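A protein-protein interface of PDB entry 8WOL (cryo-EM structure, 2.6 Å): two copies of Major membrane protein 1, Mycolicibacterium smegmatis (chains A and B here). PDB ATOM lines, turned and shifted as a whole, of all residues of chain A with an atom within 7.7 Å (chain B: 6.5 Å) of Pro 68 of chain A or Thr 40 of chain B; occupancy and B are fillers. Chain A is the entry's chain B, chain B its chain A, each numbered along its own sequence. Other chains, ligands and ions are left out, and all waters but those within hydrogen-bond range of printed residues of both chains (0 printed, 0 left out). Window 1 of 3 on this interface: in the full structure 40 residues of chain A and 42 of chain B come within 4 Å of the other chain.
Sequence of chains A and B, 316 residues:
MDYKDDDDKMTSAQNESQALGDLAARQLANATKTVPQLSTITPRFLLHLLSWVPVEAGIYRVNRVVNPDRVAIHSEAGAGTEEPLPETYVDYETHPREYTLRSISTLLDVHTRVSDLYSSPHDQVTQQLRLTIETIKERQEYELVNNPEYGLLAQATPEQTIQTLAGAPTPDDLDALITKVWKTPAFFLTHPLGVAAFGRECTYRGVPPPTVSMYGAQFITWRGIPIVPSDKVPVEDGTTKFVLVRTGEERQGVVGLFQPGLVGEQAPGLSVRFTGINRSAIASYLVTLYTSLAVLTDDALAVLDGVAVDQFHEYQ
Printed residues of chain A that touch a printed residue of chain B: Val 65, Pro 68, Lys 183, Gln 252 and Asp 299.
Hydrophobic or aromatic side chains of chain A within 4 Å of the printed part of chain B: Val 65 and Pro 68.
Along chain A the printed residues that touch a printed residue of chain B span positions 65 to 299.
Of the 9 printed residues of chain B, 4 touch a printed residue of chain A.
Hydrophobic or aromatic side chains of chain B that line the printed part of chain A: Leu 38 and Ile 41.
Along chain B the printed residues that touch a printed residue of chain A span positions 38 to 41.
O of Leu 38 of chain B is in hydrogen-bond range of NE2 of Gln 252 of chain A, at 2.8 Å.
O of Ile 41 of chain B is in hydrogen-bond range of NZ of Lys 183 of chain A (3.1 Å).
Of the printed residues of chain B, Val 65 of chain A touches Leu 38 (3.99 Å).
Of the printed residues of chain B, Pro 68 of chain A touches Leu 38 and Thr 40.
Printed residues of chain B within 4 Å of Lys 183 of chain A: Ser 39 and Ile 41.
Of the printed residues of chain B, Gln 252 of chain A touches Leu 38 (2.8 Å) and Ile 41 (3.9 Å).
Printed residues of chain B within 4 Å of Asp 299 of chain A: Ser 39.
Of chain A, only Pro 68 comes within 4 Å of Thr 40 of chain B.
Printed residues of chain A within 4 Å of Ile 41 of chain B: Lys 183 (3.1 Å) and Gln 252 (3.9 Å).
The nearest residue of chain B that does not touch Pro 68 of chain A is Ser 39 of chain B (4.2 Å).
No position is printed for both chains.
Of the 8 pairs that touch across the chains among the printed residues, none has its exchanged pair printed and touching as well.
The side-chain amino group (NZ) of Lys 183 of chain A is in salt-bridge range of the side-chain carboxylate (OD2) of Asp 299 of chain A (3.3 Å).
The side-chain hydroxyl of Thr 297 of chain A is in hydrogen-bond range of the backbone carbonyl oxygen of Gln 252 of chain A, 2.5 Å away.
The side-chain hydroxyl (OG1) of Thr 297 of chain A lies within hydrogen-bond range of the side-chain carboxylate (OD1) of Asp 299 of chain A, 3.3 Å away.
Among the printed residues, pairs that only touch across the chains: Lys 183 of chain A with Ser 39 of chain B, Asp 299 of chain A with Ser 39 of chain B, Pro 68 of chain A with Leu 38 of chain B, Pro 68 of chain A with Thr 40 of chain B, Gln 252 of chain A with Ile 41 of chain B and Val 65 of chain A with Leu 38 of chain B.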
ATOM      1  N   VAL A  65      22.377 -11.406 -15.170  1.00  0.00           N
ATOM      2  CA  VAL A  65      21.997 -10.814 -13.893  1.00  0.00           C
ATOM      3  C   VAL A  65      23.220 -10.169 -13.255  1.00  0.00           C
ATOM      4  O   VAL A  65      24.313 -10.748 -13.247  1.00  0.00           O
ATOM      5  CB  VAL A  65      21.383 -11.885 -12.972  1.00  0.00           C
ATOM      6  CG1 VAL A  65      21.168 -11.337 -11.572  1.00  0.00           C
ATOM      7  CG2 VAL A  65      20.077 -12.405 -13.556  1.00  0.00           C
ATOM      8  N   VAL A  66      23.045  -8.964 -12.715  1.00  0.00           N
ATOM      9  CA  VAL A  66      24.111  -8.244 -12.028  1.00  0.00           C
ATOM     10  C   VAL A  66      23.837  -8.269 -10.530  1.00  0.00           C
ATOM     11  O   VAL A  66      22.681  -8.202 -10.099  1.00  0.00           O
ATOM     12  CB  VAL A  66      24.249  -6.794 -12.533  1.00  0.00           C
ATOM     13  CG1 VAL A  66      24.874  -6.769 -13.914  1.00  0.00           C
ATOM     14  CG2 VAL A  66      22.899  -6.095 -12.536  1.00  0.00           C
ATOM     15  N   ASN A  67      24.909  -8.366  -9.747  1.00  0.00           N
ATOM     16  CA  ASN A  67      24.842  -8.383  -8.289  1.00  0.00           C
ATOM     17  C   ASN A  67      23.885  -9.451  -7.751  1.00  0.00           C
ATOM     18  O   ASN A  67      22.890  -9.124  -7.095  1.00  0.00           O
ATOM     19  CB  ASN A  67      24.468  -7.009  -7.752  1.00  0.00           C
ATOM     20  CG  ASN A  67      25.472  -5.940  -8.133  1.00  0.00           C
ATOM     21  OD1 ASN A  67      26.682  -6.142  -8.029  1.00  0.00           O
ATOM     22  ND2 ASN A  67      24.975  -4.790  -8.570  1.00  0.00           N
ATOM     23  N   PRO A  68      24.155 -10.734  -8.009  1.00  0.00           N
ATOM     24  CA  PRO A  68      23.273 -11.784  -7.476  1.00  0.00           C
ATOM     25  C   PRO A  68      23.274 -11.863  -5.960  1.00  0.00           C
ATOM     26  O   PRO A  68      22.340 -12.435  -5.387  1.00  0.00           O
ATOM     27  CB  PRO A  68      23.830 -13.074  -8.101  1.00  0.00           C
ATOM     28  CG  PRO A  68      24.829 -12.638  -9.131  1.00  0.00           C
ATOM     29  CD  PRO A  68      25.321 -11.301  -8.705  1.00  0.00           C
ATOM     30  N   ASP A  69      24.288 -11.308  -5.295  1.00  0.00           N
ATOM     31  CA  ASP A  69      24.373 -11.342  -3.841  1.00  0.00           C
ATOM     32  C   ASP A  69      23.453 -10.334  -3.167  1.00  0.00           C
ATOM     33  O   ASP A  69      23.313 -10.375  -1.940  1.00  0.00           O
ATOM     34  CB  ASP A  69      25.815 -11.087  -3.396  1.00  0.00           C
ATOM     35  CG  ASP A  69      26.358  -9.768  -3.910  1.00  0.00           C
ATOM     36  OD1 ASP A  69      26.641  -9.671  -5.122  1.00  0.00           O
ATOM     37  OD2 ASP A  69      26.501  -8.826  -3.102  1.00  0.00           O
ATOM     38  N   ARG A  70      22.829  -9.439  -3.928  1.00  0.00           N
ATOM     39  CA  ARG A  70      21.961  -8.412  -3.368  1.00  0.00           C
ATOM     40  C   ARG A  70      20.502  -8.839  -3.303  1.00  0.00           C
ATOM     41  O   ARG A  70      19.653  -8.031  -2.913  1.00  0.00           O
ATOM     42  CB  ARG A  70      22.088  -7.118  -4.176  1.00  0.00           C
ATOM     43  CG  ARG A  70      23.250  -6.245  -3.743  1.00  0.00           C
ATOM     44  CD  ARG A  70      23.268  -4.924  -4.489  1.00  0.00           C
ATOM     45  NE  ARG A  70      24.626  -4.421  -4.651  1.00  0.00           N
ATOM     46  CZ  ARG A  70      24.946  -3.327  -5.329  1.00  0.00           C
ATOM     47  NH1 ARG A  70      24.024  -2.589  -5.923  1.00  0.00           N
ATOM     48  NH2 ARG A  70      26.222  -2.968  -5.414  1.00  0.00           N
ATOM     49  N   VAL A  71      20.187 -10.076  -3.675  1.00  0.00           N
ATOM     50  CA  VAL A  71      18.843 -10.610  -3.484  1.00  0.00           C
ATOM     51  C   VAL A  71      18.751 -11.149  -2.062  1.00  0.00           C
ATOM     52  O   VAL A  71      19.465 -12.089  -1.697  1.00  0.00           O
ATOM     53  CB  VAL A  71      18.526 -11.702  -4.516  1.00  0.00           C
ATOM     54  CG1 VAL A  71      17.114 -12.225  -4.317  1.00  0.00           C
ATOM     55  CG2 VAL A  71      18.701 -11.163  -5.926  1.00  0.00           C
ATOM     56  N   ALA A  72      17.873 -10.555  -1.260  1.00  0.00           N
ATOM     57  CA  ALA A  72      17.793 -10.847   0.165  1.00  0.00           C
ATOM     58  C   ALA A  72      16.685 -11.855   0.435  1.00  0.00           C
ATOM     59  O   ALA A  72      15.550 -11.679  -0.020  1.00  0.00           O
ATOM     60  CB  ALA A  72      17.551  -9.570   0.972  1.00  0.00           C
ATOM     61  N   TYR A  89      14.452  -7.376  -5.623  1.00  0.00           N
ATOM     62  CA  TYR A  89      14.190  -7.619  -7.034  1.00  0.00           C
ATOM     63  C   TYR A  89      15.473  -8.147  -7.663  1.00  0.00           C
ATOM     64  O   TYR A  89      16.532  -8.174  -7.031  1.00  0.00           O
ATOM     65  CB  TYR A  89      13.704  -6.352  -7.747  1.00  0.00           C
ATOM     66  CG  TYR A  89      14.757  -5.270  -7.857  1.00  0.00           C
ATOM     67  CD1 TYR A  89      15.016  -4.415  -6.793  1.00  0.00           C
ATOM     68  CD2 TYR A  89      15.490  -5.103  -9.023  1.00  0.00           C
ATOM     69  CE1 TYR A  89      15.977  -3.428  -6.887  1.00  0.00           C
ATOM     70  CE2 TYR A  89      16.454  -4.119  -9.128  1.00  0.00           C
ATOM     71  CZ  TYR A  89      16.694  -3.283  -8.058  1.00  0.00           C
ATOM     72  OH  TYR A  89      17.652  -2.302  -8.161  1.00  0.00           O
ATOM     73  N   VAL A  90      15.373  -8.570  -8.921  1.00  0.00           N
ATOM     74  CA  VAL A  90      16.514  -9.081  -9.672  1.00  0.00           C
ATOM     75  C   VAL A  90      16.903  -8.036 -10.710  1.00  0.00           C
ATOM     76  O   VAL A  90      16.072  -7.619 -11.526  1.00  0.00           O
ATOM     77  CB  VAL A  90      16.201 -10.429 -10.337  1.00  0.00           C
ATOM     78  CG1 VAL A  90      17.454 -10.996 -10.988  1.00  0.00           C
ATOM     79  CG2 VAL A  90      15.628 -11.404  -9.318  1.00  0.00           C
ATOM     80  N   ASP A  91      18.165  -7.617 -10.680  1.00  0.00           N
ATOM     81  CA  ASP A  91      18.674  -6.577 -11.561  1.00  0.00           C
ATOM     82  C   ASP A  91      19.400  -7.187 -12.754  1.00  0.00           C
ATOM     83  O   ASP A  91      20.004  -8.259 -12.657  1.00  0.00           O
ATOM     84  CB  ASP A  91      19.616  -5.640 -10.802  1.00  0.00           C
ATOM     85  CG  ASP A  91      19.617  -4.236 -11.364  1.00  0.00           C
ATOM     86  OD1 ASP A  91      18.916  -3.995 -12.370  1.00  0.00           O
ATOM     87  OD2 ASP A  91      20.316  -3.369 -10.800  1.00  0.00           O
ATOM     88  N   LYS A 183      30.862 -27.743 -12.261  1.00  0.00           N
ATOM     89  CA  LYS A 183      29.458 -27.991 -12.585  1.00  0.00           C
ATOM     90  C   LYS A 183      29.372 -28.574 -13.991  1.00  0.00           C
ATOM     91  O   LYS A 183      29.350 -27.838 -14.981  1.00  0.00           O
ATOM     92  CB  LYS A 183      28.633 -26.714 -12.463  1.00  0.00           C
ATOM     93  CG  LYS A 183      28.981 -25.842 -11.268  1.00  0.00           C
ATOM     94  CD  LYS A 183      28.155 -24.563 -11.265  1.00  0.00           C
ATOM     95  CE  LYS A 183      28.739 -23.528 -10.317  1.00  0.00           C
ATOM     96  NZ  LYS A 183      27.926 -22.279 -10.286  1.00  0.00           N
ATOM     97  N   GLN A 252      23.612 -23.377 -19.278  1.00  0.00           N
ATOM     98  CA  GLN A 252      24.307 -22.089 -19.334  1.00  0.00           C
ATOM     99  C   GLN A 252      25.786 -22.272 -19.679  1.00  0.00           C
ATOM    100  O   GLN A 252      26.677 -21.766 -18.994  1.00  0.00           O
ATOM    101  CB  GLN A 252      24.137 -21.315 -18.023  1.00  0.00           C
ATOM    102  CG  GLN A 252      22.694 -21.203 -17.555  1.00  0.00           C
ATOM    103  CD  GLN A 252      22.533 -20.276 -16.365  1.00  0.00           C
ATOM    104  OE1 GLN A 252      21.579 -19.504 -16.290  1.00  0.00           O
ATOM    105  NE2 GLN A 252      23.467 -20.351 -15.425  1.00  0.00           N
ATOM    106  N   THR A 297      27.860 -18.196 -19.385  1.00  0.00           N
ATOM    107  CA  THR A 297      28.349 -17.882 -18.051  1.00  0.00           C
ATOM    108  C   THR A 297      29.859 -18.072 -18.004  1.00  0.00           C
ATOM    109  O   THR A 297      30.416 -18.916 -18.710  1.00  0.00           O
ATOM    110  CB  THR A 297      27.676 -18.752 -16.975  1.00  0.00           C
ATOM    111  OG1 THR A 297      27.619 -20.113 -17.420  1.00  0.00           O
ATOM    112  CG2 THR A 297      26.264 -18.254 -16.685  1.00  0.00           C
ATOM    113  N   ASP A 299      31.856 -19.272 -15.724  1.00  0.00           N
ATOM    114  CA  ASP A 299      32.367 -20.497 -15.121  1.00  0.00           C
ATOM    115  C   ASP A 299      32.203 -21.724 -16.013  1.00  0.00           C
ATOM    116  O   ASP A 299      32.419 -22.847 -15.541  1.00  0.00           O
ATOM    117  CB  ASP A 299      31.693 -20.731 -13.763  1.00  0.00           C
ATOM    118  CG  ASP A 299      30.177 -20.840 -13.860  1.00  0.00           C
ATOM    119  OD1 ASP A 299      29.640 -20.960 -14.981  1.00  0.00           O
ATOM    120  OD2 ASP A 299      29.516 -20.802 -12.801  1.00  0.00           O
ATOM    121  N   LEU B  38      21.900 -16.564 -14.671  1.00  0.00           N
ATOM    122  CA  LEU B  38      22.272 -16.447 -13.269  1.00  0.00           C
ATOM    123  C   LEU B  38      23.515 -17.292 -13.017  1.00  0.00           C
ATOM    124  O   LEU B  38      23.506 -18.504 -13.259  1.00  0.00           O
ATOM    125  CB  LEU B  38      21.121 -16.886 -12.366  1.00  0.00           C
ATOM    126  CG  LEU B  38      21.258 -16.576 -10.875  1.00  0.00           C
ATOM    127  CD1 LEU B  38      21.800 -15.169 -10.666  1.00  0.00           C
ATOM    128  CD2 LEU B  38      19.925 -16.750 -10.169  1.00  0.00           C
ATOM    129  N   SER B  39      24.580 -16.652 -12.536  1.00  0.00           N
ATOM    130  CA  SER B  39      25.849 -17.336 -12.322  1.00  0.00           C
ATOM    131  C   SER B  39      25.898 -18.113 -11.014  1.00  0.00           C
ATOM    132  O   SER B  39      26.834 -18.894 -10.814  1.00  0.00           O
ATOM    133  CB  SER B  39      27.002 -16.329 -12.360  1.00  0.00           C
ATOM    134  OG  SER B  39      27.004 -15.508 -11.206  1.00  0.00           O
ATOM    135  N   THR B  40      24.926 -17.925 -10.125  1.00  0.00           N
ATOM    136  CA  THR B  40      24.903 -18.619  -8.846  1.00  0.00           C
ATOM    137  C   THR B  40      24.125 -19.927  -8.893  1.00  0.00           C
ATOM    138  O   THR B  40      23.976 -20.577  -7.854  1.00  0.00           O
ATOM    139  CB  THR B  40      24.311 -17.715  -7.760  1.00  0.00           C
ATOM    140  OG1 THR B  40      23.235 -16.945  -8.309  1.00  0.00           O
ATOM    141  CG2 THR B  40      25.374 -16.775  -7.213  1.00  0.00           C
ATOM    142  N   ILE B  41      23.627 -20.326 -10.062  1.00  0.00           N
ATOM    143  CA  ILE B  41      22.884 -21.574 -10.173  1.00  0.00           C
ATOM    144  C   ILE B  41      23.847 -22.749 -10.073  1.00  0.00           C
ATOM    145  O   ILE B  41      24.891 -22.776 -10.738  1.00  0.00           O
ATOM    146  CB  ILE B  41      22.089 -21.610 -11.486  1.00  0.00           C
ATOM    147  CG1 ILE B  41      21.066 -20.473 -11.520  1.00  0.00           C
ATOM    148  CG2 ILE B  41      21.398 -22.952 -11.661  1.00  0.00           C
ATOM    149  CD1 ILE B  41      20.180 -20.486 -12.745  1.00  0.00           C
ATOM    150  N   THR B  42      23.499 -23.722  -9.245  1.00  0.00           N
ATOM    151  CA  THR B  42      24.274 -24.932  -9.027  1.00  0.00           C
ATOM    152  C   THR B  42      23.385 -26.132  -9.305  1.00  0.00           C
ATOM    153  O   THR B  42      22.155 -26.018  -9.279  1.00  0.00           O
ATOM    154  CB  THR B  42      24.818 -25.000  -7.590  1.00  0.00           C
ATOM    155  OG1 THR B  42      23.729 -25.094  -6.663  1.00  0.00           O
ATOM    156  CG2 THR B  42      25.653 -23.767  -7.272  1.00  0.00           C
ATOM    157  N   THR B 135      16.956 -18.583  -6.571  1.00  0.00           N
ATOM    158  CA  THR B 135      17.696 -18.124  -5.398  1.00  0.00           C
ATOM    159  C   THR B 135      17.166 -18.774  -4.123  1.00  0.00           C
ATOM    160  O   THR B 135      17.940 -19.138  -3.228  1.00  0.00           O
ATOM    161  CB  THR B 135      17.626 -16.600  -5.299  1.00  0.00           C
ATOM    162  OG1 THR B 135      18.010 -16.023  -6.552  1.00  0.00           O
ATOM    163  CG2 THR B 135      18.561 -16.093  -4.214  1.00  0.00           C
ATOM    164  N   GLU B 138      18.454 -22.344  -3.931  1.00  0.00           N
ATOM    165  CA  GLU B 138      19.845 -22.342  -3.483  1.00  0.00           C
ATOM    166  C   GLU B 138      19.939 -22.086  -1.983  1.00  0.00           C
ATOM    167  O   GLU B 138      20.747 -22.715  -1.285  1.00  0.00           O
ATOM    168  CB  GLU B 138      20.661 -21.306  -4.258  1.00  0.00           C
ATOM    169  CG  GLU B 138      20.571 -21.438  -5.769  1.00  0.00           C
ATOM    170  CD  GLU B 138      21.505 -22.499  -6.318  1.00  0.00           C
ATOM    171  OE1 GLU B 138      22.541 -22.771  -5.677  1.00  0.00           O
ATOM    172  OE2 GLU B 138      21.200 -23.064  -7.389  1.00  0.00           O
ATOM    173  N   ASP B 231      29.032 -26.652  -3.101  1.00  0.00           N
ATOM    174  CA  ASP B 231      29.688 -25.420  -2.681  1.00  0.00           C
ATOM    175  C   ASP B 231      29.181 -24.903  -1.342  1.00  0.00           C
ATOM    176  O   ASP B 231      29.789 -23.982  -0.784  1.00  0.00           O
ATOM    177  CB  ASP B 231      29.511 -24.342  -3.752  1.00  0.00           C
ATOM    178  CG  ASP B 231      28.069 -24.189  -4.190  1.00  0.00           C
ATOM    179  OD1 ASP B 231      27.302 -25.167  -4.063  1.00  0.00           O
ATOM    180  OD2 ASP B 231      27.701 -23.092  -4.657  1.00  0.00           O
ATOM    181  N   LYS B 232      28.093 -25.464  -0.814  1.00  0.00           N
ATOM    182  CA  LYS B 232      27.550 -25.019   0.463  1.00  0.00           C
ATOM    183  C   LYS B 232      28.302 -25.584   1.661  1.00  0.00           C
ATOM    184  O   LYS B 232      28.106 -25.094   2.777  1.00  0.00           O
ATOM    185  CB  LYS B 232      26.069 -25.389   0.565  1.00  0.00           C
ATOM    186  CG  LYS B 232      25.233 -24.939  -0.620  1.00  0.00           C
ATOM    187  CD  LYS B 232      25.474 -23.473  -0.943  1.00  0.00           C
ATOM    188  CE  LYS B 232      24.349 -22.906  -1.788  1.00  0.00           C
ATOM    189  NZ  LYS B 232      24.455 -23.331  -3.210  1.00  0.00           N
